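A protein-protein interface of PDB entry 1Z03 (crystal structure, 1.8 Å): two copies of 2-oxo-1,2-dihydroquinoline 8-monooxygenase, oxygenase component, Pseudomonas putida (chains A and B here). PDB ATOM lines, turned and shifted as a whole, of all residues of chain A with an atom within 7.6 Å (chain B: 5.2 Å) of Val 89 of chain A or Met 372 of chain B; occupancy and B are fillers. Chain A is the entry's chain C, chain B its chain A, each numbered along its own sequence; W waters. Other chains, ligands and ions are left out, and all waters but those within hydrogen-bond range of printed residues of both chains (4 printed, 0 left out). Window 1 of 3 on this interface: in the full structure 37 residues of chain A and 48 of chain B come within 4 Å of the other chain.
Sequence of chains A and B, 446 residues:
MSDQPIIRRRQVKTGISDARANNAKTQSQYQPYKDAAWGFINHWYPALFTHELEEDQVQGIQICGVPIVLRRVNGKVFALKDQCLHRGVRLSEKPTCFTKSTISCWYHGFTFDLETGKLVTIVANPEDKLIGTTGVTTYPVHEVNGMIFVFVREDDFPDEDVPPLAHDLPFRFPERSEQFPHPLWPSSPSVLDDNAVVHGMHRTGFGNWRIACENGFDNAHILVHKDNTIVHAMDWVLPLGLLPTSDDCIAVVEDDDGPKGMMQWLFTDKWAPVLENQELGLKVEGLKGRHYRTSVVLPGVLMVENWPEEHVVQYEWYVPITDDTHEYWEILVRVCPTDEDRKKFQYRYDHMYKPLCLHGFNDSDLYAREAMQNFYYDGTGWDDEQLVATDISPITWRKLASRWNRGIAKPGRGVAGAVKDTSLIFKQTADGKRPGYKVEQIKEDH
The side-chain hydroxyl (OH) of Tyr 376 of chain B lies within hydrogen-bond range of the guanidinium group (NE) of Arg 87 of chain A (2.8 Å). SD of Met 372 of chain B lies within hydrogen-bond range of NE of Arg 87 of chain A (3.6 Å).
O of Arg 90 of chain A is in hydrogen-bond range of NE1 of Trp 106 of chain A (3.0 Å). The side-chain sulfur of Cys 105 of chain A lies close to the backbone NH of Tyr 107 of chain A (3.6 Å). The backbone NH (N) of Cys 84 of chain A is in hydrogen-bond range of the backbone carbonyl oxygen (O) of Val 89 of chain A (2.9 Å). OE2 of Glu 93 of chain A is in salt-bridge range of NE of Arg 90 of chain A (2.9 Å).
Gln 83 of chain A touches Phe 375 of chain B. Arg 87 of chain A touches Ile 211 of chain B (NH1 to CD1, 3.8 Å). N of Gly 88 of chain A touches CD2 of Phe 375 of chain B, at 3.5 Å. CA of Val 89 of chain A touches O of Ala 371 of chain B (3.5 Å). Val 89 of chain A touches Met 372 of chain B (CG1 to CB, 3.8 Å). CZ3 of Trp 106 of chain A touches CA of Ala 368 of chain B, at 3.6 Å. Ala 371 of chain B touches Trp 106 of chain A. Tyr 107 of chain A touches Ala 368 of chain B. Tyr 107 of chain A touches Met 372 of chain B. Phe 375 of chain B touches Gly 414 of chain A.
Asp 82 of chain A touches none of the printed residues of chain B. His 86 of chain A touches none of the printed residues of chain B. Of chain B, only Ala 371 and Met 372 come within 4 Å of Val 89 of chain A. Of the printed residues of chain B, Trp 106 of chain A touches Ala 368 (3.6 Å) and Ala 371 (3.5 Å). Of the printed residues of chain B, Leu 424 of chain A touches Glu 370 (3.4 Å) and Gln 373 (3.99 Å). Of the printed residues of chain A, Glu 370 of chain B touches Leu 424 (3.4 Å). Met 372 of chain B touches just these residues of chain A: Arg 87, Val 89 and Tyr 107. Printed residues of chain A within 4 Å of Gln 373 of chain B: Leu 424. Of the printed residues of chain A, Tyr 376 of chain B touches Arg 87 (2.8 Å).
Of the 19 printed residues of chain A, 9 touch a printed residue of chain B. Hydrophobic or aromatic side chains of chain A within 4 Å of the printed part of chain B: Val 89, Trp 106, Tyr 107 and Leu 424. Hydrophobic or aromatic side chains of chain B that line the printed part of chain A: Ile 211, Ala 368, Ala 371, Met 372, Phe 375 and Tyr 376. Along chain B the printed residues that touch a printed residue of chain A span positions 211 to 376. Among the printed residues, 17 pairs touch across the chains. Among the printed residues, no Asp or Glu carboxylate lies within 4 Å of a Lys or Arg side-chain nitrogen of the other chain.
No position is printed for both chains.
Water W3 lies within hydrogen-bond range of the side-chain carboxylate (OE2) of Glu 93 of chain A (2.5 Å), the backbone carbonyl oxygen (O) of Ala 371 of chain B (2.6 Å) and the backbone NH (N) of Arg 90 of chain A (2.9 Å). Water W2 lies within hydrogen-bond range of O of Ala 371 of chain B (2.7 Å), O of Gly 88 of chain A (3.0 Å) and N of Phe 375 of chain B (3.4 Å). Water W1 lies within hydrogen-bond range of NH1 of Arg 90 of chain A (3.4 Å) and OD1 of Asn 374 of chain B (3.4 Å). Water W4 lies within hydrogen-bond range of the side-chain carboxylate of Glu 93 of chain A (3.4 Å) and the backbone NH of Ala 371 of chain B (3.5 Å).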
ATOM      1  N   LYS A  81     -16.940  -1.299   1.862  1.00  0.00           N
ATOM      2  CA  LYS A  81     -17.581  -2.379   2.593  1.00  0.00           C
ATOM      3  C   LYS A  81     -19.061  -2.050   2.657  1.00  0.00           C
ATOM      4  O   LYS A  81     -19.445  -0.924   2.998  1.00  0.00           O
ATOM      5  CB  LYS A  81     -17.010  -2.515   4.004  1.00  0.00           C
ATOM      6  CG  LYS A  81     -17.515  -3.761   4.719  1.00  0.00           C
ATOM      7  CD  LYS A  81     -16.985  -3.866   6.127  1.00  0.00           C
ATOM      8  CE  LYS A  81     -15.492  -4.134   6.150  1.00  0.00           C
ATOM      9  NZ  LYS A  81     -15.004  -4.178   7.554  1.00  0.00           N
ATOM     10  N   ASP A  82     -19.892  -3.028   2.313  1.00  0.00           N
ATOM     11  CA  ASP A  82     -21.335  -2.834   2.310  1.00  0.00           C
ATOM     12  C   ASP A  82     -21.882  -3.022   3.718  1.00  0.00           C
ATOM     13  O   ASP A  82     -22.707  -3.912   3.975  1.00  0.00           O
ATOM     14  CB  ASP A  82     -21.991  -3.829   1.351  1.00  0.00           C
ATOM     15  CG  ASP A  82     -23.416  -3.443   0.989  1.00  0.00           C
ATOM     16  OD1 ASP A  82     -24.100  -4.273   0.362  1.00  0.00           O
ATOM     17  OD2 ASP A  82     -23.853  -2.316   1.316  1.00  0.00           O
ATOM     18  N   GLN A  83     -21.400  -2.184   4.630  1.00  0.00           N
ATOM     19  CA  GLN A  83     -21.823  -2.229   6.020  1.00  0.00           C
ATOM     20  C   GLN A  83     -21.691  -0.868   6.680  1.00  0.00           C
ATOM     21  O   GLN A  83     -20.580  -0.401   6.946  1.00  0.00           O
ATOM     22  CB  GLN A  83     -20.980  -3.232   6.806  1.00  0.00           C
ATOM     23  CG  GLN A  83     -21.367  -3.321   8.278  1.00  0.00           C
ATOM     24  CD  GLN A  83     -20.340  -4.069   9.112  1.00  0.00           C
ATOM     25  OE1 GLN A  83     -19.205  -3.608   9.280  1.00  0.00           O
ATOM     26  NE2 GLN A  83     -20.733  -5.228   9.645  1.00  0.00           N
ATOM     27  N   CYS A  84     -22.824  -0.229   6.940  1.00  0.00           N
ATOM     28  CA  CYS A  84     -22.812   1.065   7.595  1.00  0.00           C
ATOM     29  C   CYS A  84     -22.211   0.845   8.976  1.00  0.00           C
ATOM     30  O   CYS A  84     -22.652  -0.041   9.707  1.00  0.00           O
ATOM     31  CB  CYS A  84     -24.233   1.598   7.717  1.00  0.00           C
ATOM     32  SG  CYS A  84     -24.316   3.225   8.428  1.00  0.00           S
ATOM     33  N   LEU A  85     -21.203   1.639   9.332  1.00  0.00           N
ATOM     34  CA  LEU A  85     -20.549   1.494  10.623  1.00  0.00           C
ATOM     35  C   LEU A  85     -21.403   1.949  11.811  1.00  0.00           C
ATOM     36  O   LEU A  85     -21.035   1.725  12.967  1.00  0.00           O
ATOM     37  CB  LEU A  85     -19.191   2.217  10.595  1.00  0.00           C
ATOM     38  CG  LEU A  85     -19.095   3.731  10.347  1.00  0.00           C
ATOM     39  CD1 LEU A  85     -19.468   4.487  11.623  1.00  0.00           C
ATOM     40  CD2 LEU A  85     -17.669   4.084   9.920  1.00  0.00           C
ATOM     41  N   HIS A  86     -22.552   2.564  11.530  1.00  0.00           N
ATOM     42  CA  HIS A  86     -23.456   3.016  12.589  1.00  0.00           C
ATOM     43  C   HIS A  86     -24.181   1.812  13.194  1.00  0.00           C
ATOM     44  O   HIS A  86     -23.907   1.412  14.322  1.00  0.00           O
ATOM     45  CB  HIS A  86     -24.499   3.994  12.051  1.00  0.00           C
ATOM     46  CG  HIS A  86     -25.451   4.487  13.096  1.00  0.00           C
ATOM     47  ND1 HIS A  86     -26.789   4.704  12.847  1.00  0.00           N
ATOM     48  CD2 HIS A  86     -25.258   4.804  14.398  1.00  0.00           C
ATOM     49  CE1 HIS A  86     -27.381   5.127  13.949  1.00  0.00           C
ATOM     50  NE2 HIS A  86     -26.473   5.196  14.906  1.00  0.00           N
ATOM     51  N   ARG A  87     -25.117   1.227  12.450  1.00  0.00           N
ATOM     52  CA  ARG A  87     -25.822   0.073  12.984  1.00  0.00           C
ATOM     53  C   ARG A  87     -25.877  -1.135  12.051  1.00  0.00           C
ATOM     54  O   ARG A  87     -26.812  -1.941  12.083  1.00  0.00           O
ATOM     55  CB  ARG A  87     -27.207   0.495  13.481  1.00  0.00           C
ATOM     56  CG  ARG A  87     -27.084   1.520  14.611  1.00  0.00           C
ATOM     57  CD  ARG A  87     -28.374   1.758  15.358  1.00  0.00           C
ATOM     58  NE  ARG A  87     -28.830   0.553  16.045  1.00  0.00           N
ATOM     59  CZ  ARG A  87     -29.898   0.509  16.832  1.00  0.00           C
ATOM     60  NH1 ARG A  87     -30.247  -0.630  17.415  1.00  0.00           N
ATOM     61  NH2 ARG A  87     -30.610   1.610  17.035  1.00  0.00           N
ATOM     62  N   GLY A  88     -24.846  -1.239  11.217  1.00  0.00           N
ATOM     63  CA  GLY A  88     -24.676  -2.376  10.331  1.00  0.00           C
ATOM     64  C   GLY A  88     -25.583  -2.714   9.168  1.00  0.00           C
ATOM     65  O   GLY A  88     -25.533  -3.854   8.705  1.00  0.00           O
ATOM     66  N   VAL A  89     -26.397  -1.786   8.671  1.00  0.00           N
ATOM     67  CA  VAL A  89     -27.243  -2.131   7.533  1.00  0.00           C
ATOM     68  C   VAL A  89     -26.393  -2.088   6.262  1.00  0.00           C
ATOM     69  O   VAL A  89     -25.325  -1.472   6.238  1.00  0.00           O
ATOM     70  CB  VAL A  89     -28.435  -1.144   7.366  1.00  0.00           C
ATOM     71  CG1 VAL A  89     -29.238  -1.050   8.657  1.00  0.00           C
ATOM     72  CG2 VAL A  89     -27.922   0.218   6.948  1.00  0.00           C
ATOM     73  N   ARG A  90     -26.857  -2.756   5.213  1.00  0.00           N
ATOM     74  CA  ARG A  90     -26.147  -2.744   3.939  1.00  0.00           C
ATOM     75  C   ARG A  90     -26.538  -1.487   3.175  1.00  0.00           C
ATOM     76  O   ARG A  90     -27.726  -1.222   2.951  1.00  0.00           O
ATOM     77  CB  ARG A  90     -26.495  -3.978   3.101  1.00  0.00           C
ATOM     78  CG  ARG A  90     -25.789  -5.235   3.556  1.00  0.00           C
ATOM     79  CD  ARG A  90     -26.107  -6.441   2.671  1.00  0.00           C
ATOM     80  NE  ARG A  90     -27.524  -6.787   2.707  1.00  0.00           N
ATOM     81  CZ  ARG A  90     -28.009  -7.997   2.438  1.00  0.00           C
ATOM     82  NH1 ARG A  90     -29.316  -8.213   2.497  1.00  0.00           N
ATOM     83  NH2 ARG A  90     -27.187  -8.991   2.117  1.00  0.00           N
ATOM     84  N   LEU A  91     -25.533  -0.717   2.774  1.00  0.00           N
ATOM     85  CA  LEU A  91     -25.752   0.519   2.036  1.00  0.00           C
ATOM     86  C   LEU A  91     -26.383   0.260   0.668  1.00  0.00           C
ATOM     87  O   LEU A  91     -27.094   1.110   0.138  1.00  0.00           O
ATOM     88  CB  LEU A  91     -24.416   1.248   1.844  1.00  0.00           C
ATOM     89  CG  LEU A  91     -23.586   1.532   3.101  1.00  0.00           C
ATOM     90  CD1 LEU A  91     -22.177   1.936   2.691  1.00  0.00           C
ATOM     91  CD2 LEU A  91     -24.254   2.617   3.938  1.00  0.00           C
ATOM     92  N   SER A  92     -26.127  -0.920   0.110  1.00  0.00           N
ATOM     93  CA  SER A  92     -26.626  -1.280  -1.218  1.00  0.00           C
ATOM     94  C   SER A  92     -28.090  -1.699  -1.312  1.00  0.00           C
ATOM     95  O   SER A  92     -28.600  -1.900  -2.415  1.00  0.00           O
ATOM     96  CB  SER A  92     -25.791  -2.413  -1.793  1.00  0.00           C
ATOM     97  OG  SER A  92     -26.113  -3.617  -1.122  1.00  0.00           O
ATOM     98  N   GLU A  93     -28.760  -1.850  -0.174  1.00  0.00           N
ATOM     99  CA  GLU A  93     -30.160  -2.264  -0.191  1.00  0.00           C
ATOM    100  C   GLU A  93     -31.114  -1.195  -0.695  1.00  0.00           C
ATOM    101  O   GLU A  93     -32.146  -1.508  -1.271  1.00  0.00           O
ATOM    102  CB  GLU A  93     -30.583  -2.737   1.192  1.00  0.00           C
ATOM    103  CG  GLU A  93     -30.153  -4.165   1.466  1.00  0.00           C
ATOM    104  CD  GLU A  93     -30.716  -4.683   2.750  1.00  0.00           C
ATOM    105  OE1 GLU A  93     -31.874  -4.348   3.057  1.00  0.00           O
ATOM    106  OE2 GLU A  93     -30.008  -5.431   3.447  1.00  0.00           O
ATOM    107  N   CYS A 105     -25.973   6.188   3.889  1.00  0.00           N
ATOM    108  CA  CYS A 105     -26.802   5.117   4.403  1.00  0.00           C
ATOM    109  C   CYS A 105     -28.224   5.670   4.426  1.00  0.00           C
ATOM    110  O   CYS A 105     -28.478   6.740   4.971  1.00  0.00           O
ATOM    111  CB  CYS A 105     -26.376   4.717   5.816  1.00  0.00           C
ATOM    112  SG  CYS A 105     -27.400   3.387   6.474  1.00  0.00           S
ATOM    113  N   TRP A 106     -29.144   4.930   3.823  1.00  0.00           N
ATOM    114  CA  TRP A 106     -30.548   5.321   3.736  1.00  0.00           C
ATOM    115  C   TRP A 106     -31.295   5.323   5.059  1.00  0.00           C
ATOM    116  O   TRP A 106     -32.424   5.811   5.133  1.00  0.00           O
ATOM    117  CB  TRP A 106     -31.277   4.381   2.783  1.00  0.00           C
ATOM    118  CG  TRP A 106     -30.907   2.947   3.029  1.00  0.00           C
ATOM    119  CD1 TRP A 106     -29.810   2.279   2.534  1.00  0.00           C
ATOM    120  CD2 TRP A 106     -31.570   2.031   3.903  1.00  0.00           C
ATOM    121  NE1 TRP A 106     -29.754   1.006   3.054  1.00  0.00           N
ATOM    122  CE2 TRP A 106     -30.822   0.829   3.899  1.00  0.00           C
ATOM    123  CE3 TRP A 106     -32.726   2.108   4.692  1.00  0.00           C
ATOM    124  CZ2 TRP A 106     -31.192  -0.284   4.658  1.00  0.00           C
ATOM    125  CZ3 TRP A 106     -33.093   1.001   5.447  1.00  0.00           C
ATOM    126  CH2 TRP A 106     -32.327  -0.180   5.424  1.00  0.00           C
ATOM    127  N   TYR A 107     -30.681   4.773   6.100  1.00  0.00           N
ATOM    128  CA  TYR A 107     -31.342   4.692   7.390  1.00  0.00           C
ATOM    129  C   TYR A 107     -31.215   5.941   8.261  1.00  0.00           C
ATOM    130  O   TYR A 107     -32.224   6.595   8.526  1.00  0.00           O
ATOM    131  CB  TYR A 107     -30.841   3.461   8.144  1.00  0.00           C
ATOM    132  CG  TYR A 107     -31.809   2.904   9.159  1.00  0.00           C
ATOM    133  CD1 TYR A 107     -31.572   1.666   9.754  1.00  0.00           C
ATOM    134  CD2 TYR A 107     -32.966   3.597   9.520  1.00  0.00           C
ATOM    135  CE1 TYR A 107     -32.457   1.130  10.675  1.00  0.00           C
ATOM    136  CE2 TYR A 107     -33.860   3.070  10.446  1.00  0.00           C
ATOM    137  CZ  TYR A 107     -33.599   1.835  11.019  1.00  0.00           C
ATOM    138  OH  TYR A 107     -34.472   1.288  11.937  1.00  0.00           O
ATOM    139  N   HIS A 108     -30.001   6.277   8.705  1.00  0.00           N
ATOM    140  CA  HIS A 108     -29.815   7.456   9.558  1.00  0.00           C
ATOM    141  C   HIS A 108     -28.900   8.502   8.927  1.00  0.00           C
ATOM    142  O   HIS A 108     -28.478   9.458   9.587  1.00  0.00           O
ATOM    143  CB  HIS A 108     -29.279   7.061  10.944  1.00  0.00           C
ATOM    144  CG  HIS A 108     -30.084   5.996  11.629  1.00  0.00           C
ATOM    145  ND1 HIS A 108     -29.734   4.661  11.598  1.00  0.00           N
ATOM    146  CD2 HIS A 108     -31.221   6.066  12.360  1.00  0.00           C
ATOM    147  CE1 HIS A 108     -30.619   3.957  12.281  1.00  0.00           C
ATOM    148  NE2 HIS A 108     -31.532   4.785  12.754  1.00  0.00           N
ATOM    149  N   GLY A 414     -21.615 -10.712  12.121  1.00  0.00           N
ATOM    150  CA  GLY A 414     -22.486  -9.556  12.009  1.00  0.00           C
ATOM    151  C   GLY A 414     -22.807  -9.130  10.591  1.00  0.00           C
ATOM    152  O   GLY A 414     -23.154  -7.976  10.353  1.00  0.00           O
ATOM    153  N   LEU A 424     -34.818 -14.640   8.784  1.00  0.00           N
ATOM    154  CA  LEU A 424     -34.771 -13.884   7.524  1.00  0.00           C
ATOM    155  C   LEU A 424     -34.474 -14.832   6.360  1.00  0.00           C
ATOM    156  O   LEU A 424     -35.055 -14.712   5.271  1.00  0.00           O
ATOM    157  CB  LEU A 424     -33.686 -12.803   7.580  1.00  0.00           C
ATOM    158  CG  LEU A 424     -34.062 -11.476   8.249  1.00  0.00           C
ATOM    159  CD1 LEU A 424     -32.818 -10.630   8.474  1.00  0.00           C
ATOM    160  CD2 LEU A 424     -35.081 -10.736   7.369  1.00  0.00           C
ATOM    161  N   ILE B 211     -34.374  -4.847  18.081  1.00  0.00           N
ATOM    162  CA  ILE B 211     -33.975  -4.070  16.921  1.00  0.00           C
ATOM    163  C   ILE B 211     -35.184  -3.455  16.210  1.00  0.00           C
ATOM    164  O   ILE B 211     -35.088  -2.371  15.629  1.00  0.00           O
ATOM    165  CB  ILE B 211     -33.175  -4.952  15.940  1.00  0.00           C
ATOM    166  CG1 ILE B 211     -31.876  -5.422  16.605  1.00  0.00           C
ATOM    167  CG2 ILE B 211     -32.918  -4.209  14.655  1.00  0.00           C
ATOM    168  CD1 ILE B 211     -30.990  -4.304  17.120  1.00  0.00           C
ATOM    169  N   ALA B 368     -36.458  -1.419   7.018  1.00  0.00           N
ATOM    170  CA  ALA B 368     -35.336  -0.782   7.704  1.00  0.00           C
ATOM    171  C   ALA B 368     -34.919  -1.648   8.893  1.00  0.00           C
ATOM    172  O   ALA B 368     -33.727  -1.901   9.090  1.00  0.00           O
ATOM    173  CB  ALA B 368     -35.731   0.619   8.183  1.00  0.00           C
ATOM    174  N   ARG B 369     -35.906  -2.101   9.673  1.00  0.00           N
ATOM    175  CA  ARG B 369     -35.655  -2.938  10.850  1.00  0.00           C
ATOM    176  C   ARG B 369     -35.015  -4.257  10.447  1.00  0.00           C
ATOM    177  O   ARG B 369     -34.087  -4.736  11.094  1.00  0.00           O
ATOM    178  CB  ARG B 369     -36.956  -3.255  11.580  1.00  0.00           C
ATOM    179  CG  ARG B 369     -37.730  -2.064  12.065  1.00  0.00           C
ATOM    180  CD  ARG B 369     -39.109  -2.513  12.469  1.00  0.00           C
ATOM    181  NE  ARG B 369     -39.969  -1.386  12.803  1.00  0.00           N
ATOM    182  CZ  ARG B 369     -41.277  -1.363  12.581  1.00  0.00           C
ATOM    183  NH1 ARG B 369     -41.981  -0.291  12.919  1.00  0.00           N
ATOM    184  NH2 ARG B 369     -41.875  -2.408  12.016  1.00  0.00           N
ATOM    185  N   GLU B 370     -35.529  -4.849   9.375  1.00  0.00           N
ATOM    186  CA  GLU B 370     -35.005  -6.118   8.888  1.00  0.00           C
ATOM    187  C   GLU B 370     -33.540  -6.009   8.470  1.00  0.00           C
ATOM    188  O   GLU B 370     -32.721  -6.863   8.799  1.00  0.00           O
ATOM    189  CB  GLU B 370     -35.831  -6.600   7.695  1.00  0.00           C
ATOM    190  CG  GLU B 370     -36.742  -7.775   7.976  1.00  0.00           C
ATOM    191  CD  GLU B 370     -37.503  -8.234   6.743  1.00  0.00           C
ATOM    192  OE1 GLU B 370     -36.901  -8.276   5.651  1.00  0.00           O
ATOM    193  OE2 GLU B 370     -38.701  -8.569   6.862  1.00  0.00           O
ATOM    194  N   ALA B 371     -33.211  -4.950   7.742  1.00  0.00           N
ATOM    195  CA  ALA B 371     -31.846  -4.751   7.254  1.00  0.00           C
ATOM    196  C   ALA B 371     -30.774  -4.599   8.332  1.00  0.00           C
ATOM    197  O   ALA B 371     -29.587  -4.703   8.045  1.00  0.00           O
ATOM    198  CB  ALA B 371     -31.813  -3.540   6.339  1.00  0.00           C
ATOM    199  N   MET B 372     -31.194  -4.363   9.567  1.00  0.00           N
ATOM    200  CA  MET B 372     -30.277  -4.166  10.681  1.00  0.00           C
ATOM    201  C   MET B 372     -30.067  -5.430  11.519  1.00  0.00           C
ATOM    202  O   MET B 372     -29.105  -5.536  12.280  1.00  0.00           O
ATOM    203  CB  MET B 372     -30.842  -3.021  11.533  1.00  0.00           C
ATOM    204  CG  MET B 372     -30.133  -2.704  12.818  1.00  0.00           C
ATOM    205  SD  MET B 372     -30.729  -1.100  13.482  1.00  0.00           S
ATOM    206  CE  MET B 372     -32.522  -1.241  13.361  1.00  0.00           C
ATOM    207  N   GLN B 373     -30.955  -6.403  11.350  1.00  0.00           N
ATOM    208  CA  GLN B 373     -30.910  -7.642  12.121  1.00  0.00           C
ATOM    209  C   GLN B 373     -29.648  -8.498  12.040  1.00  0.00           C
ATOM    210  O   GLN B 373     -29.205  -9.023  13.062  1.00  0.00           O
ATOM    211  CB  GLN B 373     -32.127  -8.495  11.776  1.00  0.00           C
ATOM    212  CG  GLN B 373     -33.463  -7.801  12.030  1.00  0.00           C
ATOM    213  CD  GLN B 373     -33.803  -7.674  13.506  1.00  0.00           C
ATOM    214  OE1 GLN B 373     -33.012  -8.028  14.375  1.00  0.00           O
ATOM    215  NE2 GLN B 373     -34.991  -7.162  13.794  1.00  0.00           N
ATOM    216  N   ASN B 374     -29.071  -8.655  10.846  1.00  0.00           N
ATOM    217  CA  ASN B 374     -27.855  -9.469  10.673  1.00  0.00           C
ATOM    218  C   ASN B 374     -26.653  -8.973  11.477  1.00  0.00           C
ATOM    219  O   ASN B 374     -25.805  -9.755  11.899  1.00  0.00           O
ATOM    220  CB  ASN B 374     -27.458  -9.534   9.189  1.00  0.00           C
ATOM    221  CG  ASN B 374     -28.250 -10.578   8.410  1.00  0.00           C
ATOM    222  OD1 ASN B 374     -28.245 -10.587   7.177  1.00  0.00           O
ATOM    223  ND2 ASN B 374     -28.922 -11.468   9.125  1.00  0.00           N
ATOM    224  N   PHE B 375     -26.574  -7.668  11.675  1.00  0.00           N
ATOM    225  CA  PHE B 375     -25.470  -7.076  12.422  1.00  0.00           C
ATOM    226  C   PHE B 375     -25.515  -7.468  13.904  1.00  0.00           C
ATOM    227  O   PHE B 375     -24.473  -7.652  14.551  1.00  0.00           O
ATOM    228  CB  PHE B 375     -25.531  -5.545  12.274  1.00  0.00           C
ATOM    229  CG  PHE B 375     -24.344  -4.817  12.857  1.00  0.00           C
ATOM    230  CD1 PHE B 375     -23.046  -5.228  12.572  1.00  0.00           C
ATOM    231  CD2 PHE B 375     -24.526  -3.676  13.638  1.00  0.00           C
ATOM    232  CE1 PHE B 375     -21.950  -4.518  13.048  1.00  0.00           C
ATOM    233  CE2 PHE B 375     -23.424  -2.958  14.120  1.00  0.00           C
ATOM    234  CZ  PHE B 375     -22.138  -3.382  13.822  1.00  0.00           C
ATOM    235  N   TYR B 376     -26.724  -7.625  14.425  1.00  0.00           N
ATOM    236  CA  TYR B 376     -26.920  -7.928  15.833  1.00  0.00           C
ATOM    237  C   TYR B 376     -27.167  -9.371  16.272  1.00  0.00           C
ATOM    238  O   TYR B 376     -26.788  -9.736  17.393  1.00  0.00           O
ATOM    239  CB  TYR B 376     -28.076  -7.076  16.368  1.00  0.00           C
ATOM    240  CG  TYR B 376     -27.808  -5.586  16.372  1.00  0.00           C
ATOM    241  CD1 TYR B 376     -27.288  -4.954  17.506  1.00  0.00           C
ATOM    242  CD2 TYR B 376     -28.048  -4.814  15.238  1.00  0.00           C
ATOM    243  CE1 TYR B 376     -27.016  -3.593  17.504  1.00  0.00           C
ATOM    244  CE2 TYR B 376     -27.778  -3.450  15.223  1.00  0.00           C
ATOM    245  CZ  TYR B 376     -27.264  -2.849  16.360  1.00  0.00           C
ATOM    246  OH  TYR B 376     -26.998  -1.503  16.352  1.00  0.00           O
HETATM  247  O   HOH W   1     -30.092  -8.123   5.774  1.00  0.00           O
HETATM  248  O   HOH W   2     -27.419  -6.131   8.719  1.00  0.00           O
HETATM  249  O   HOH W   3     -28.802  -4.855   5.569  1.00  0.00           O
HETATM  250  O   HOH W   4     -34.837  -5.025   4.670  1.00  0.00           O
